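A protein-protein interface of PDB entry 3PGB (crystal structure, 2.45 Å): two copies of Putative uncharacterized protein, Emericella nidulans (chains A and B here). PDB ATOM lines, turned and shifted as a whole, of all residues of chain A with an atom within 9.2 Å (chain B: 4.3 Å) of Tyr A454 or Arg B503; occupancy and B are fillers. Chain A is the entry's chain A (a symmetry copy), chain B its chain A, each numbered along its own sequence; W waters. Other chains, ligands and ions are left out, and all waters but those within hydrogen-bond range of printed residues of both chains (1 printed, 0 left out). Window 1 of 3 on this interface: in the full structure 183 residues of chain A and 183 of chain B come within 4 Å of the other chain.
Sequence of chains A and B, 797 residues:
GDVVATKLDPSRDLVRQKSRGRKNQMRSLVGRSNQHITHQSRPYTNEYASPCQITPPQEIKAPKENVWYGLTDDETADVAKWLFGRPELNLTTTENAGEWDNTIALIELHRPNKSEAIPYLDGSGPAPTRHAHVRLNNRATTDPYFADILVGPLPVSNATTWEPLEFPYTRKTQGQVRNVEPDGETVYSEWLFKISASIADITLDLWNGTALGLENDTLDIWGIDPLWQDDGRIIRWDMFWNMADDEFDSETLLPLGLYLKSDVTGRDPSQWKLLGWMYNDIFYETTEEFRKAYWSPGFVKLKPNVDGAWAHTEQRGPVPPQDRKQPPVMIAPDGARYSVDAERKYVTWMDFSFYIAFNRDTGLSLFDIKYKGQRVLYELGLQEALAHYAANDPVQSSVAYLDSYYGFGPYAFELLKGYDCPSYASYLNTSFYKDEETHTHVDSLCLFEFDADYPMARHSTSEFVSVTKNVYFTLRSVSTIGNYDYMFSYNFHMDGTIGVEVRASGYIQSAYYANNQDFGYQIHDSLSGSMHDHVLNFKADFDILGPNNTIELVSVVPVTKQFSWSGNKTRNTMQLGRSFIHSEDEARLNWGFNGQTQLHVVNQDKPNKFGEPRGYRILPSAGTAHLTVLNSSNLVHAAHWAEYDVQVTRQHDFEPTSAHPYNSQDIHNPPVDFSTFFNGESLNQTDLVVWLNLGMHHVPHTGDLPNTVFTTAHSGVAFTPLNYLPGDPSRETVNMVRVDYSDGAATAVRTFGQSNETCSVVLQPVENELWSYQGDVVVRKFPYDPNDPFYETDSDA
Hydrophobic or aromatic side chains of chain B within 4 Å of the printed part of chain A: Met B487 and Phe B710.
Of the 22 printed residues of chain A, 8 touch a printed residue of chain B.
Among the printed residues, 15 pairs touch across the chains.
Position printed for both chains: 501.
Of the 15 pairs that touch across the chains among the printed residues, none has its exchanged pair printed and touching as well.
The guanidinium group (NH2) of Arg B503 lies within hydrogen-bond range of a ring nitrogen (NE2) of His B714 (3.4 Å).
The backbone carbonyl oxygen (O) of Phe B710 is in hydrogen-bond range of the guanidinium group (NH1) of Arg B503 (2.6 Å).
The backbone carbonyl oxygen of Thr A468 is in hydrogen-bond range of the backbone NH of Met A456, at 2.8 Å.
N of Ala A452 is in hydrogen-bond range of O of Asn A470 (2.9 Å).
The backbone carbonyl oxygen (O) of Thr B711 is in hydrogen-bond range of the guanidinium group (NH1) of Arg B503, at 3.3 Å.
The side-chain hydroxyl (OG1) of Thr A497 sits at hydrogen-bond distance from the side-chain carboxylate (OD1) of Asp A495 (2.9 Å).
Among the printed residues, pairs that only touch across the chains: Met A456 with Thr B711 (2.9 Å), Pro A455 with Met B487 (3.2 Å), Pro A455 with Phe B710 (3.2 Å), Arg A458 with Phe B710 (3.5 Å), Asn A470 with Thr B711 (3.7 Å), Tyr A454 with Thr B711 (3.8 Å), Tyr A454 with Arg B476 (3.9 Å), Tyr A454 with Phe B710 (3.9 Å), Ala A457 with Phe B710 (3.9 Å) and Tyr A454 with Met B487 (3.99 Å).
Of the printed residues of chain B, Tyr A454 touches Arg B476 (3.9 Å), Met B487 (3.99 Å), Arg B503 (3.3 Å), Phe B710 (3.9 Å) and Thr B711 (3.8 Å).
Of the printed residues of chain B, Pro A455 touches Met B487 (3.2 Å) and Phe B710 (3.2 Å).
Printed residues of chain B within 4 Å of Ala A457: Phe B710 (3.9 Å).
Printed residues of chain B within 4 Å of Arg A458: Asp B485 (2.7 Å) and Phe B710 (3.5 Å).
Arg B503 touches just one residue of chain A: Tyr A454.
No residue of chain A comes within 4 Å of Ala B504.
The nearest printed residue of chain B that does not touch Tyr A454 is Glu B501 (6.0 Å).
The nearest residue of chain A that does not touch Arg B503 is Pro A455 (5.7 Å).
The nearest printed residue of chain B that does not touch Asp A495 is Phe B710 (6.5 Å).
Water W1 lies within hydrogen-bond range of OD2 of Asp A453 and NH2 of Arg B476.
N of Phe B710 lies within hydrogen-bond range of O of Met A456, 2.7 Å away.
OD2 of Asp B485 is in salt-bridge range of NH1 of Arg A458, at 2.7 Å.
NH1 of Arg B503 lies within hydrogen-bond range of OH of Tyr A454 (3.3 Å).
The side-chain hydroxyl of Thr B711 sits at hydrogen-bond distance from the side-chain carboxylate of Asp A495, 2.6 Å away.
The guanidinium group of Arg B476 is in salt-bridge range of the side-chain carboxylate of Asp A453 (3.8 Å).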
ATOM      1  N   MET A 330      14.943   7.947  -9.903  1.00  0.00           N
ATOM      2  CA  MET A 330      15.211   7.616 -11.298  1.00  0.00           C
ATOM      3  C   MET A 330      14.346   6.418 -11.649  1.00  0.00           C
ATOM      4  O   MET A 330      14.304   5.446 -10.899  1.00  0.00           O
ATOM      5  CB  MET A 330      16.700   7.292 -11.488  1.00  0.00           C
ATOM      6  CG  MET A 330      17.174   7.186 -12.941  1.00  0.00           C
ATOM      7  SD  MET A 330      17.258   8.747 -13.854  1.00  0.00           S
ATOM      8  CE  MET A 330      18.904   9.332 -13.466  1.00  0.00           C
ATOM      9  N   PHE A 450      21.705   5.449 -16.767  1.00  0.00           N
ATOM     10  CA  PHE A 450      21.463   6.567 -15.869  1.00  0.00           C
ATOM     11  C   PHE A 450      21.535   7.858 -16.657  1.00  0.00           C
ATOM     12  O   PHE A 450      22.516   8.108 -17.349  1.00  0.00           O
ATOM     13  CB  PHE A 450      22.490   6.569 -14.730  1.00  0.00           C
ATOM     14  CG  PHE A 450      22.124   7.464 -13.584  1.00  0.00           C
ATOM     15  CD1 PHE A 450      21.394   6.973 -12.509  1.00  0.00           C
ATOM     16  CD2 PHE A 450      22.507   8.799 -13.579  1.00  0.00           C
ATOM     17  CE1 PHE A 450      21.051   7.800 -11.449  1.00  0.00           C
ATOM     18  CE2 PHE A 450      22.167   9.634 -12.519  1.00  0.00           C
ATOM     19  CZ  PHE A 450      21.443   9.134 -11.455  1.00  0.00           C
ATOM     20  N   ASP A 451      20.476   8.658 -16.574  1.00  0.00           N
ATOM     21  CA  ASP A 451      20.437   9.965 -17.223  1.00  0.00           C
ATOM     22  C   ASP A 451      21.139  10.965 -16.318  1.00  0.00           C
ATOM     23  O   ASP A 451      20.601  11.348 -15.287  1.00  0.00           O
ATOM     24  CB  ASP A 451      18.991  10.390 -17.473  1.00  0.00           C
ATOM     25  CG  ASP A 451      18.883  11.703 -18.234  1.00  0.00           C
ATOM     26  OD1 ASP A 451      17.744  12.130 -18.509  1.00  0.00           O
ATOM     27  OD2 ASP A 451      19.914  12.313 -18.562  1.00  0.00           O
ATOM     28  N   ALA A 452      22.347  11.372 -16.710  1.00  0.00           N
ATOM     29  CA  ALA A 452      23.173  12.272 -15.901  1.00  0.00           C
ATOM     30  C   ALA A 452      22.444  13.572 -15.624  1.00  0.00           C
ATOM     31  O   ALA A 452      21.644  14.028 -16.445  1.00  0.00           O
ATOM     32  CB  ALA A 452      24.487  12.553 -16.600  1.00  0.00           C
ATOM     33  N   ASP A 453      22.732  14.178 -14.477  1.00  0.00           N
ATOM     34  CA  ASP A 453      22.097  15.444 -14.107  1.00  0.00           C
ATOM     35  C   ASP A 453      22.503  16.625 -15.008  1.00  0.00           C
ATOM     36  O   ASP A 453      21.959  17.719 -14.867  1.00  0.00           O
ATOM     37  CB  ASP A 453      22.344  15.775 -12.622  1.00  0.00           C
ATOM     38  CG  ASP A 453      23.760  16.263 -12.332  1.00  0.00           C
ATOM     39  OD1 ASP A 453      24.706  15.878 -13.047  1.00  0.00           O
ATOM     40  OD2 ASP A 453      23.925  17.020 -11.346  1.00  0.00           O
ATOM     41  N   TYR A 454      23.450  16.399 -15.919  1.00  0.00           N
ATOM     42  CA  TYR A 454      23.886  17.412 -16.881  1.00  0.00           C
ATOM     43  C   TYR A 454      23.864  16.802 -18.282  1.00  0.00           C
ATOM     44  O   TYR A 454      24.108  15.612 -18.434  1.00  0.00           O
ATOM     45  CB  TYR A 454      25.308  17.900 -16.533  1.00  0.00           C
ATOM     46  CG  TYR A 454      26.389  16.839 -16.686  1.00  0.00           C
ATOM     47  CD1 TYR A 454      26.722  15.992 -15.636  1.00  0.00           C
ATOM     48  CD2 TYR A 454      27.072  16.682 -17.890  1.00  0.00           C
ATOM     49  CE1 TYR A 454      27.712  15.017 -15.780  1.00  0.00           C
ATOM     50  CE2 TYR A 454      28.049  15.716 -18.046  1.00  0.00           C
ATOM     51  CZ  TYR A 454      28.367  14.887 -16.990  1.00  0.00           C
ATOM     52  OH  TYR A 454      29.343  13.933 -17.148  1.00  0.00           O
ATOM     53  N   PRO A 455      23.597  17.619 -19.313  1.00  0.00           N
ATOM     54  CA  PRO A 455      23.525  17.110 -20.678  1.00  0.00           C
ATOM     55  C   PRO A 455      24.902  16.776 -21.235  1.00  0.00           C
ATOM     56  O   PRO A 455      25.907  17.218 -20.690  1.00  0.00           O
ATOM     57  CB  PRO A 455      22.915  18.281 -21.447  1.00  0.00           C
ATOM     58  CG  PRO A 455      23.411  19.469 -20.743  1.00  0.00           C
ATOM     59  CD  PRO A 455      23.486  19.085 -19.283  1.00  0.00           C
ATOM     60  N   MET A 456      24.935  16.000 -22.312  1.00  0.00           N
ATOM     61  CA  MET A 456      26.183  15.646 -22.984  1.00  0.00           C
ATOM     62  C   MET A 456      26.796  16.861 -23.696  1.00  0.00           C
ATOM     63  O   MET A 456      28.000  17.114 -23.600  1.00  0.00           O
ATOM     64  CB  MET A 456      25.917  14.525 -24.002  1.00  0.00           C
ATOM     65  CG  MET A 456      27.094  14.153 -24.910  1.00  0.00           C
ATOM     66  SD  MET A 456      28.306  13.111 -24.080  1.00  0.00           S
ATOM     67  CE  MET A 456      29.010  14.299 -22.980  1.00  0.00           C
ATOM     68  N   ALA A 457      25.957  17.603 -24.413  1.00  0.00           N
ATOM     69  CA  ALA A 457      26.416  18.723 -25.229  1.00  0.00           C
ATOM     70  C   ALA A 457      25.282  19.713 -25.470  1.00  0.00           C
ATOM     71  O   ALA A 457      24.103  19.367 -25.369  1.00  0.00           O
ATOM     72  CB  ALA A 457      26.959  18.209 -26.557  1.00  0.00           C
ATOM     73  N   ARG A 458      25.644  20.950 -25.787  1.00  0.00           N
ATOM     74  CA  ARG A 458      24.654  21.968 -26.103  1.00  0.00           C
ATOM     75  C   ARG A 458      25.279  23.082 -26.888  1.00  0.00           C
ATOM     76  O   ARG A 458      26.500  23.222 -26.899  1.00  0.00           O
ATOM     77  CB  ARG A 458      24.060  22.560 -24.830  1.00  0.00           C
ATOM     78  CG  ARG A 458      24.979  23.535 -24.122  1.00  0.00           C
ATOM     79  CD  ARG A 458      24.411  24.028 -22.791  1.00  0.00           C
ATOM     80  NE  ARG A 458      22.971  24.267 -22.841  1.00  0.00           N
ATOM     81  CZ  ARG A 458      22.384  25.267 -23.492  1.00  0.00           C
ATOM     82  NH1 ARG A 458      23.098  26.157 -24.187  1.00  0.00           N
ATOM     83  NH2 ARG A 458      21.067  25.374 -23.461  1.00  0.00           N
ATOM     84  N   VAL A 467      20.408  20.688 -27.629  1.00  0.00           N
ATOM     85  CA  VAL A 467      20.976  19.946 -26.501  1.00  0.00           C
ATOM     86  C   VAL A 467      20.915  18.432 -26.729  1.00  0.00           C
ATOM     87  O   VAL A 467      19.969  17.932 -27.342  1.00  0.00           O
ATOM     88  CB  VAL A 467      20.240  20.266 -25.186  1.00  0.00           C
ATOM     89  CG1 VAL A 467      20.943  19.595 -24.009  1.00  0.00           C
ATOM     90  CG2 VAL A 467      20.152  21.765 -24.966  1.00  0.00           C
ATOM     91  N   THR A 468      21.939  17.726 -26.247  1.00  0.00           N
ATOM     92  CA  THR A 468      21.986  16.263 -26.271  1.00  0.00           C
ATOM     93  C   THR A 468      22.027  15.754 -24.835  1.00  0.00           C
ATOM     94  O   THR A 468      22.787  16.272 -24.012  1.00  0.00           O
ATOM     95  CB  THR A 468      23.246  15.743 -26.996  1.00  0.00           C
ATOM     96  OG1 THR A 468      23.278  16.243 -28.338  1.00  0.00           O
ATOM     97  CG2 THR A 468      23.260  14.229 -27.032  1.00  0.00           C
ATOM     98  N   LYS A 469      21.212  14.748 -24.532  1.00  0.00           N
ATOM     99  CA  LYS A 469      21.193  14.174 -23.193  1.00  0.00           C
ATOM    100  C   LYS A 469      22.446  13.348 -22.950  1.00  0.00           C
ATOM    101  O   LYS A 469      23.049  12.842 -23.891  1.00  0.00           O
ATOM    102  CB  LYS A 469      19.957  13.294 -22.986  1.00  0.00           C
ATOM    103  CG  LYS A 469      18.623  14.028 -23.071  1.00  0.00           C
ATOM    104  CD  LYS A 469      17.487  13.230 -22.413  1.00  0.00           C
ATOM    105  CE  LYS A 469      17.039  13.828 -21.078  1.00  0.00           C
ATOM    106  NZ  LYS A 469      18.139  14.028 -20.099  1.00  0.00           N
ATOM    107  N   ASN A 470      22.832  13.224 -21.685  1.00  0.00           N
ATOM    108  CA  ASN A 470      23.956  12.382 -21.284  1.00  0.00           C
ATOM    109  C   ASN A 470      23.430  11.116 -20.612  1.00  0.00           C
ATOM    110  O   ASN A 470      23.326  11.035 -19.377  1.00  0.00           O
ATOM    111  CB  ASN A 470      24.894  13.152 -20.343  1.00  0.00           C
ATOM    112  CG  ASN A 470      26.131  12.364 -19.959  1.00  0.00           C
ATOM    113  OD1 ASN A 470      26.460  11.354 -20.571  1.00  0.00           O
ATOM    114  ND2 ASN A 470      26.825  12.830 -18.935  1.00  0.00           N
ATOM    115  N   VAL A 471      23.085  10.132 -21.435  1.00  0.00           N
ATOM    116  CA  VAL A 471      22.648   8.835 -20.939  1.00  0.00           C
ATOM    117  C   VAL A 471      23.820   7.863 -21.016  1.00  0.00           C
ATOM    118  O   VAL A 471      24.382   7.654 -22.097  1.00  0.00           O
ATOM    119  CB  VAL A 471      21.453   8.295 -21.743  1.00  0.00           C
ATOM    120  CG1 VAL A 471      20.977   6.975 -21.151  1.00  0.00           C
ATOM    121  CG2 VAL A 471      20.324   9.313 -21.757  1.00  0.00           C
ATOM    122  N   TYR A 472      24.193   7.290 -19.873  1.00  0.00           N
ATOM    123  CA  TYR A 472      25.355   6.410 -19.788  1.00  0.00           C
ATOM    124  C   TYR A 472      25.049   5.087 -19.079  1.00  0.00           C
ATOM    125  O   TYR A 472      24.077   4.990 -18.329  1.00  0.00           O
ATOM    126  CB  TYR A 472      26.517   7.134 -19.097  1.00  0.00           C
ATOM    127  CG  TYR A 472      26.285   7.503 -17.647  1.00  0.00           C
ATOM    128  CD1 TYR A 472      26.719   6.678 -16.618  1.00  0.00           C
ATOM    129  CD2 TYR A 472      25.659   8.696 -17.306  1.00  0.00           C
ATOM    130  CE1 TYR A 472      26.507   7.018 -15.285  1.00  0.00           C
ATOM    131  CE2 TYR A 472      25.451   9.044 -15.985  1.00  0.00           C
ATOM    132  CZ  TYR A 472      25.875   8.201 -14.980  1.00  0.00           C
ATOM    133  OH  TYR A 472      25.666   8.558 -13.671  1.00  0.00           O
ATOM    134  N   ASN A 491      31.879   2.854 -16.069  1.00  0.00           N
ATOM    135  CA  ASN A 491      30.961   3.711 -16.811  1.00  0.00           C
ATOM    136  C   ASN A 491      31.237   3.646 -18.304  1.00  0.00           C
ATOM    137  O   ASN A 491      32.388   3.560 -18.715  1.00  0.00           O
ATOM    138  CB  ASN A 491      31.125   5.169 -16.369  1.00  0.00           C
ATOM    139  CG  ASN A 491      30.681   5.401 -14.950  1.00  0.00           C
ATOM    140  OD1 ASN A 491      29.633   4.906 -14.531  1.00  0.00           O
ATOM    141  ND2 ASN A 491      31.464   6.164 -14.199  1.00  0.00           N
ATOM    142  N   HIS A 493      29.935   5.852 -21.875  1.00  0.00           N
ATOM    143  CA  HIS A 493      29.201   7.031 -22.324  1.00  0.00           C
ATOM    144  C   HIS A 493      29.055   7.107 -23.836  1.00  0.00           C
ATOM    145  O   HIS A 493      29.804   6.467 -24.577  1.00  0.00           O
ATOM    146  CB  HIS A 493      29.900   8.275 -21.817  1.00  0.00           C
ATOM    147  CG  HIS A 493      29.968   8.357 -20.325  1.00  0.00           C
ATOM    148  ND1 HIS A 493      30.910   7.675 -19.585  1.00  0.00           N
ATOM    149  CD2 HIS A 493      29.206   9.035 -19.435  1.00  0.00           C
ATOM    150  CE1 HIS A 493      30.726   7.934 -18.303  1.00  0.00           C
ATOM    151  NE2 HIS A 493      29.696   8.754 -18.184  1.00  0.00           N
ATOM    152  N   ASP A 495      29.785   9.413 -25.860  1.00  0.00           N
ATOM    153  CA  ASP A 495      30.953  10.000 -26.541  1.00  0.00           C
ATOM    154  C   ASP A 495      32.121   9.008 -26.668  1.00  0.00           C
ATOM    155  O   ASP A 495      33.175   9.348 -27.198  1.00  0.00           O
ATOM    156  CB  ASP A 495      31.418  11.272 -25.812  1.00  0.00           C
ATOM    157  CG  ASP A 495      31.909  11.001 -24.386  1.00  0.00           C
ATOM    158  OD1 ASP A 495      32.547  11.900 -23.803  1.00  0.00           O
ATOM    159  OD2 ASP A 495      31.667   9.900 -23.848  1.00  0.00           O
ATOM    160  N   THR A 497      33.517   7.460 -24.011  1.00  0.00           N
ATOM    161  CA  THR A 497      34.345   7.530 -22.816  1.00  0.00           C
ATOM    162  C   THR A 497      34.046   6.368 -21.864  1.00  0.00           C
ATOM    163  O   THR A 497      32.894   6.121 -21.507  1.00  0.00           O
ATOM    164  CB  THR A 497      34.144   8.872 -22.090  1.00  0.00           C
ATOM    165  OG1 THR A 497      34.559   9.949 -22.951  1.00  0.00           O
ATOM    166  CG2 THR A 497      34.945   8.916 -20.799  1.00  0.00           C
ATOM    167  N   GLU A 501      35.900   3.992 -11.664  1.00  0.00           N
ATOM    168  CA  GLU A 501      35.802   4.734 -10.407  1.00  0.00           C
ATOM    169  C   GLU A 501      35.821   3.830  -9.186  1.00  0.00           C
ATOM    170  O   GLU A 501      35.384   2.678  -9.236  1.00  0.00           O
ATOM    171  CB  GLU A 501      34.492   5.515 -10.350  1.00  0.00           C
ATOM    172  CG  GLU A 501      34.419   6.726 -11.247  1.00  0.00           C
ATOM    173  CD  GLU A 501      33.056   7.398 -11.177  1.00  0.00           C
ATOM    174  OE1 GLU A 501      32.490   7.510 -10.060  1.00  0.00           O
ATOM    175  OE2 GLU A 501      32.546   7.805 -12.243  1.00  0.00           O
ATOM    176  N   SER A 621      39.965  11.723 -14.143  1.00  0.00           N
ATOM    177  CA  SER A 621      38.762  12.548 -14.131  1.00  0.00           C
ATOM    178  C   SER A 621      38.329  12.952 -12.723  1.00  0.00           C
ATOM    179  O   SER A 621      37.884  14.083 -12.512  1.00  0.00           O
ATOM    180  CB  SER A 621      37.612  11.822 -14.835  1.00  0.00           C
ATOM    181  OG  SER A 621      37.749  11.958 -16.240  1.00  0.00           O
ATOM    182  N   ARG B 476      21.706  26.085 -10.908  1.00  0.00           N
ATOM    183  CA  ARG B 476      22.446  26.097 -12.163  1.00  0.00           C
ATOM    184  C   ARG B 476      22.108  27.255 -13.097  1.00  0.00           C
ATOM    185  O   ARG B 476      20.972  27.711 -13.172  1.00  0.00           O
ATOM    186  CB  ARG B 476      22.241  24.772 -12.884  1.00  0.00           C
ATOM    187  CG  ARG B 476      22.815  24.706 -14.278  1.00  0.00           C
ATOM    188  CD  ARG B 476      22.723  23.305 -14.815  1.00  0.00           C
ATOM    189  NE  ARG B 476      23.454  22.344 -13.990  1.00  0.00           N
ATOM    190  CZ  ARG B 476      23.324  21.023 -14.079  1.00  0.00           C
ATOM    191  NH1 ARG B 476      22.482  20.477 -14.956  1.00  0.00           N
ATOM    192  NH2 ARG B 476      24.041  20.234 -13.280  1.00  0.00           N
ATOM    193  N   ASP B 485      29.724  27.495 -24.541  1.00  0.00           N
ATOM    194  CA  ASP B 485      28.631  27.249 -23.601  1.00  0.00           C
ATOM    195  C   ASP B 485      29.207  26.801 -22.276  1.00  0.00           C
ATOM    196  O   ASP B 485      29.677  25.675 -22.149  1.00  0.00           O
ATOM    197  CB  ASP B 485      27.659  26.196 -24.125  1.00  0.00           C
ATOM    198  CG  ASP B 485      26.825  26.707 -25.275  1.00  0.00           C
ATOM    199  OD1 ASP B 485      27.409  27.055 -26.321  1.00  0.00           O
ATOM    200  OD2 ASP B 485      25.589  26.767 -25.136  1.00  0.00           O
ATOM    201  N   TYR B 486      29.183  27.701 -21.299  1.00  0.00           N
ATOM    202  CA  TYR B 486      29.618  27.389 -19.952  1.00  0.00           C
ATOM    203  C   TYR B 486      28.406  27.039 -19.113  1.00  0.00           C
ATOM    204  O   TYR B 486      27.483  27.836 -19.017  1.00  0.00           O
ATOM    205  CB  TYR B 486      30.330  28.586 -19.329  1.00  0.00           C
ATOM    206  CG  TYR B 486      31.642  28.928 -19.986  1.00  0.00           C
ATOM    207  CD1 TYR B 486      32.761  28.112 -19.816  1.00  0.00           C
ATOM    208  CD2 TYR B 486      31.778  30.076 -20.762  1.00  0.00           C
ATOM    209  CE1 TYR B 486      33.987  28.431 -20.411  1.00  0.00           C
ATOM    210  CE2 TYR B 486      32.991  30.406 -21.360  1.00  0.00           C
ATOM    211  CZ  TYR B 486      34.094  29.580 -21.182  1.00  0.00           C
ATOM    212  OH  TYR B 486      35.299  29.904 -21.779  1.00  0.00           O
ATOM    213  N   MET B 487      28.406  25.851 -18.515  1.00  0.00           N
ATOM    214  CA  MET B 487      27.336  25.449 -17.606  1.00  0.00           C
ATOM    215  C   MET B 487      27.881  25.461 -16.188  1.00  0.00           C
ATOM    216  O   MET B 487      28.757  24.670 -15.858  1.00  0.00           O
ATOM    217  CB  MET B 487      26.810  24.052 -17.971  1.00  0.00           C
ATOM    218  CG  MET B 487      25.784  23.472 -16.983  1.00  0.00           C
ATOM    219  SD  MET B 487      25.239  21.794 -17.407  1.00  0.00           S
ATOM    220  CE  MET B 487      23.896  22.164 -18.543  1.00  0.00           C
ATOM    221  N   GLU B 501      31.105  23.832  -9.763  1.00  0.00           N
ATOM    222  CA  GLU B 501      31.530  23.166 -10.995  1.00  0.00           C
ATOM    223  C   GLU B 501      31.324  24.027 -12.231  1.00  0.00           C
ATOM    224  O   GLU B 501      30.421  24.865 -12.285  1.00  0.00           O
ATOM    225  CB  GLU B 501      30.723  21.889 -11.216  1.00  0.00           C
ATOM    226  CG  GLU B 501      31.062  20.741 -10.298  1.00  0.00           C
ATOM    227  CD  GLU B 501      30.163  19.539 -10.542  1.00  0.00           C
ATOM    228  OE1 GLU B 501      29.874  19.227 -11.726  1.00  0.00           O
ATOM    229  OE2 GLU B 501      29.736  18.913  -9.549  1.00  0.00           O
ATOM    230  N   VAL B 502      32.159  23.780 -13.235  1.00  0.00           N
ATOM    231  CA  VAL B 502      31.898  24.263 -14.583  1.00  0.00           C
ATOM    232  C   VAL B 502      32.134  23.136 -15.577  1.00  0.00           C
ATOM    233  O   VAL B 502      33.048  22.326 -15.417  1.00  0.00           O
ATOM    234  CB  VAL B 502      32.781  25.469 -14.952  1.00  0.00           C
ATOM    235  CG1 VAL B 502      34.253  25.079 -14.948  1.00  0.00           C
ATOM    236  CG2 VAL B 502      32.365  26.033 -16.313  1.00  0.00           C
ATOM    237  N   ARG B 503      31.279  23.072 -16.589  1.00  0.00           N
ATOM    238  CA  ARG B 503      31.551  22.254 -17.753  1.00  0.00           C
ATOM    239  C   ARG B 503      31.446  23.122 -19.002  1.00  0.00           C
ATOM    240  O   ARG B 503      30.759  24.147 -19.003  1.00  0.00           O
ATOM    241  CB  ARG B 503      30.600  21.059 -17.825  1.00  0.00           C
ATOM    242  CG  ARG B 503      30.625  20.167 -16.610  1.00  0.00           C
ATOM    243  CD  ARG B 503      29.568  19.077 -16.683  1.00  0.00           C
ATOM    244  NE  ARG B 503      29.733  18.111 -15.602  1.00  0.00           N
ATOM    245  CZ  ARG B 503      30.461  17.001 -15.663  1.00  0.00           C
ATOM    246  NH1 ARG B 503      31.113  16.659 -16.771  1.00  0.00           N
ATOM    247  NH2 ARG B 503      30.536  16.214 -14.596  1.00  0.00           N
ATOM    248  N   ALA B 504      32.143  22.706 -20.056  1.00  0.00           N
ATOM    249  CA  ALA B 504      32.179  23.447 -21.309  1.00  0.00           C
ATOM    250  C   ALA B 504      31.653  22.595 -22.455  1.00  0.00           C
ATOM    251  O   ALA B 504      31.867  21.385 -22.495  1.00  0.00           O
ATOM    252  CB  ALA B 504      33.588  23.910 -21.613  1.00  0.00           C
ATOM    253  N   PHE B 710      30.381  18.030 -22.630  1.00  0.00           N
ATOM    254  CA  PHE B 710      30.418  18.333 -21.199  1.00  0.00           C
ATOM    255  C   PHE B 710      31.034  17.225 -20.341  1.00  0.00           C
ATOM    256  O   PHE B 710      31.478  17.483 -19.224  1.00  0.00           O
ATOM    257  CB  PHE B 710      29.001  18.600 -20.674  1.00  0.00           C
ATOM    258  CG  PHE B 710      28.437  19.950 -21.049  1.00  0.00           C
ATOM    259  CD1 PHE B 710      29.128  21.118 -20.757  1.00  0.00           C
ATOM    260  CD2 PHE B 710      27.182  20.050 -21.644  1.00  0.00           C
ATOM    261  CE1 PHE B 710      28.602  22.359 -21.085  1.00  0.00           C
ATOM    262  CE2 PHE B 710      26.643  21.289 -21.971  1.00  0.00           C
ATOM    263  CZ  PHE B 710      27.354  22.449 -21.691  1.00  0.00           C
ATOM    264  N   THR B 711      31.032  15.993 -20.839  1.00  0.00           N
ATOM    265  CA  THR B 711      31.525  14.863 -20.059  1.00  0.00           C
ATOM    266  C   THR B 711      32.967  15.058 -19.621  1.00  0.00           C
ATOM    267  O   THR B 711      33.314  14.812 -18.476  1.00  0.00           O
ATOM    268  CB  THR B 711      31.467  13.554 -20.867  1.00  0.00           C
ATOM    269  OG1 THR B 711      31.744  13.842 -22.242  1.00  0.00           O
ATOM    270  CG2 THR B 711      30.103  12.887 -20.728  1.00  0.00           C
ATOM    271  N   ALA B 713      35.039  17.991 -20.672  1.00  0.00           N
ATOM    272  CA  ALA B 713      35.373  19.396 -20.423  1.00  0.00           C
ATOM    273  C   ALA B 713      34.754  19.826 -19.090  1.00  0.00           C
ATOM    274  O   ALA B 713      33.673  20.404 -19.048  1.00  0.00           O
ATOM    275  CB  ALA B 713      34.884  20.274 -21.563  1.00  0.00           C
ATOM    276  N   HIS B 714      35.461  19.544 -18.005  1.00  0.00           N
ATOM    277  CA  HIS B 714      34.896  19.620 -16.663  1.00  0.00           C
ATOM    278  C   HIS B 714      35.981  19.991 -15.659  1.00  0.00           C
ATOM    279  O   HIS B 714      37.134  19.591 -15.794  1.00  0.00           O
ATOM    280  CB  HIS B 714      34.257  18.272 -16.316  1.00  0.00           C
ATOM    281  CG  HIS B 714      33.733  18.172 -14.917  1.00  0.00           C
ATOM    282  ND1 HIS B 714      32.983  19.165 -14.327  1.00  0.00           N
ATOM    283  CD2 HIS B 714      33.806  17.169 -14.011  1.00  0.00           C
ATOM    284  CE1 HIS B 714      32.642  18.790 -13.107  1.00  0.00           C
ATOM    285  NE2 HIS B 714      33.129  17.583 -12.890  1.00  0.00           N
HETATM  286  O   HOH W   1      25.093  19.741 -10.193  1.00  0.00           O
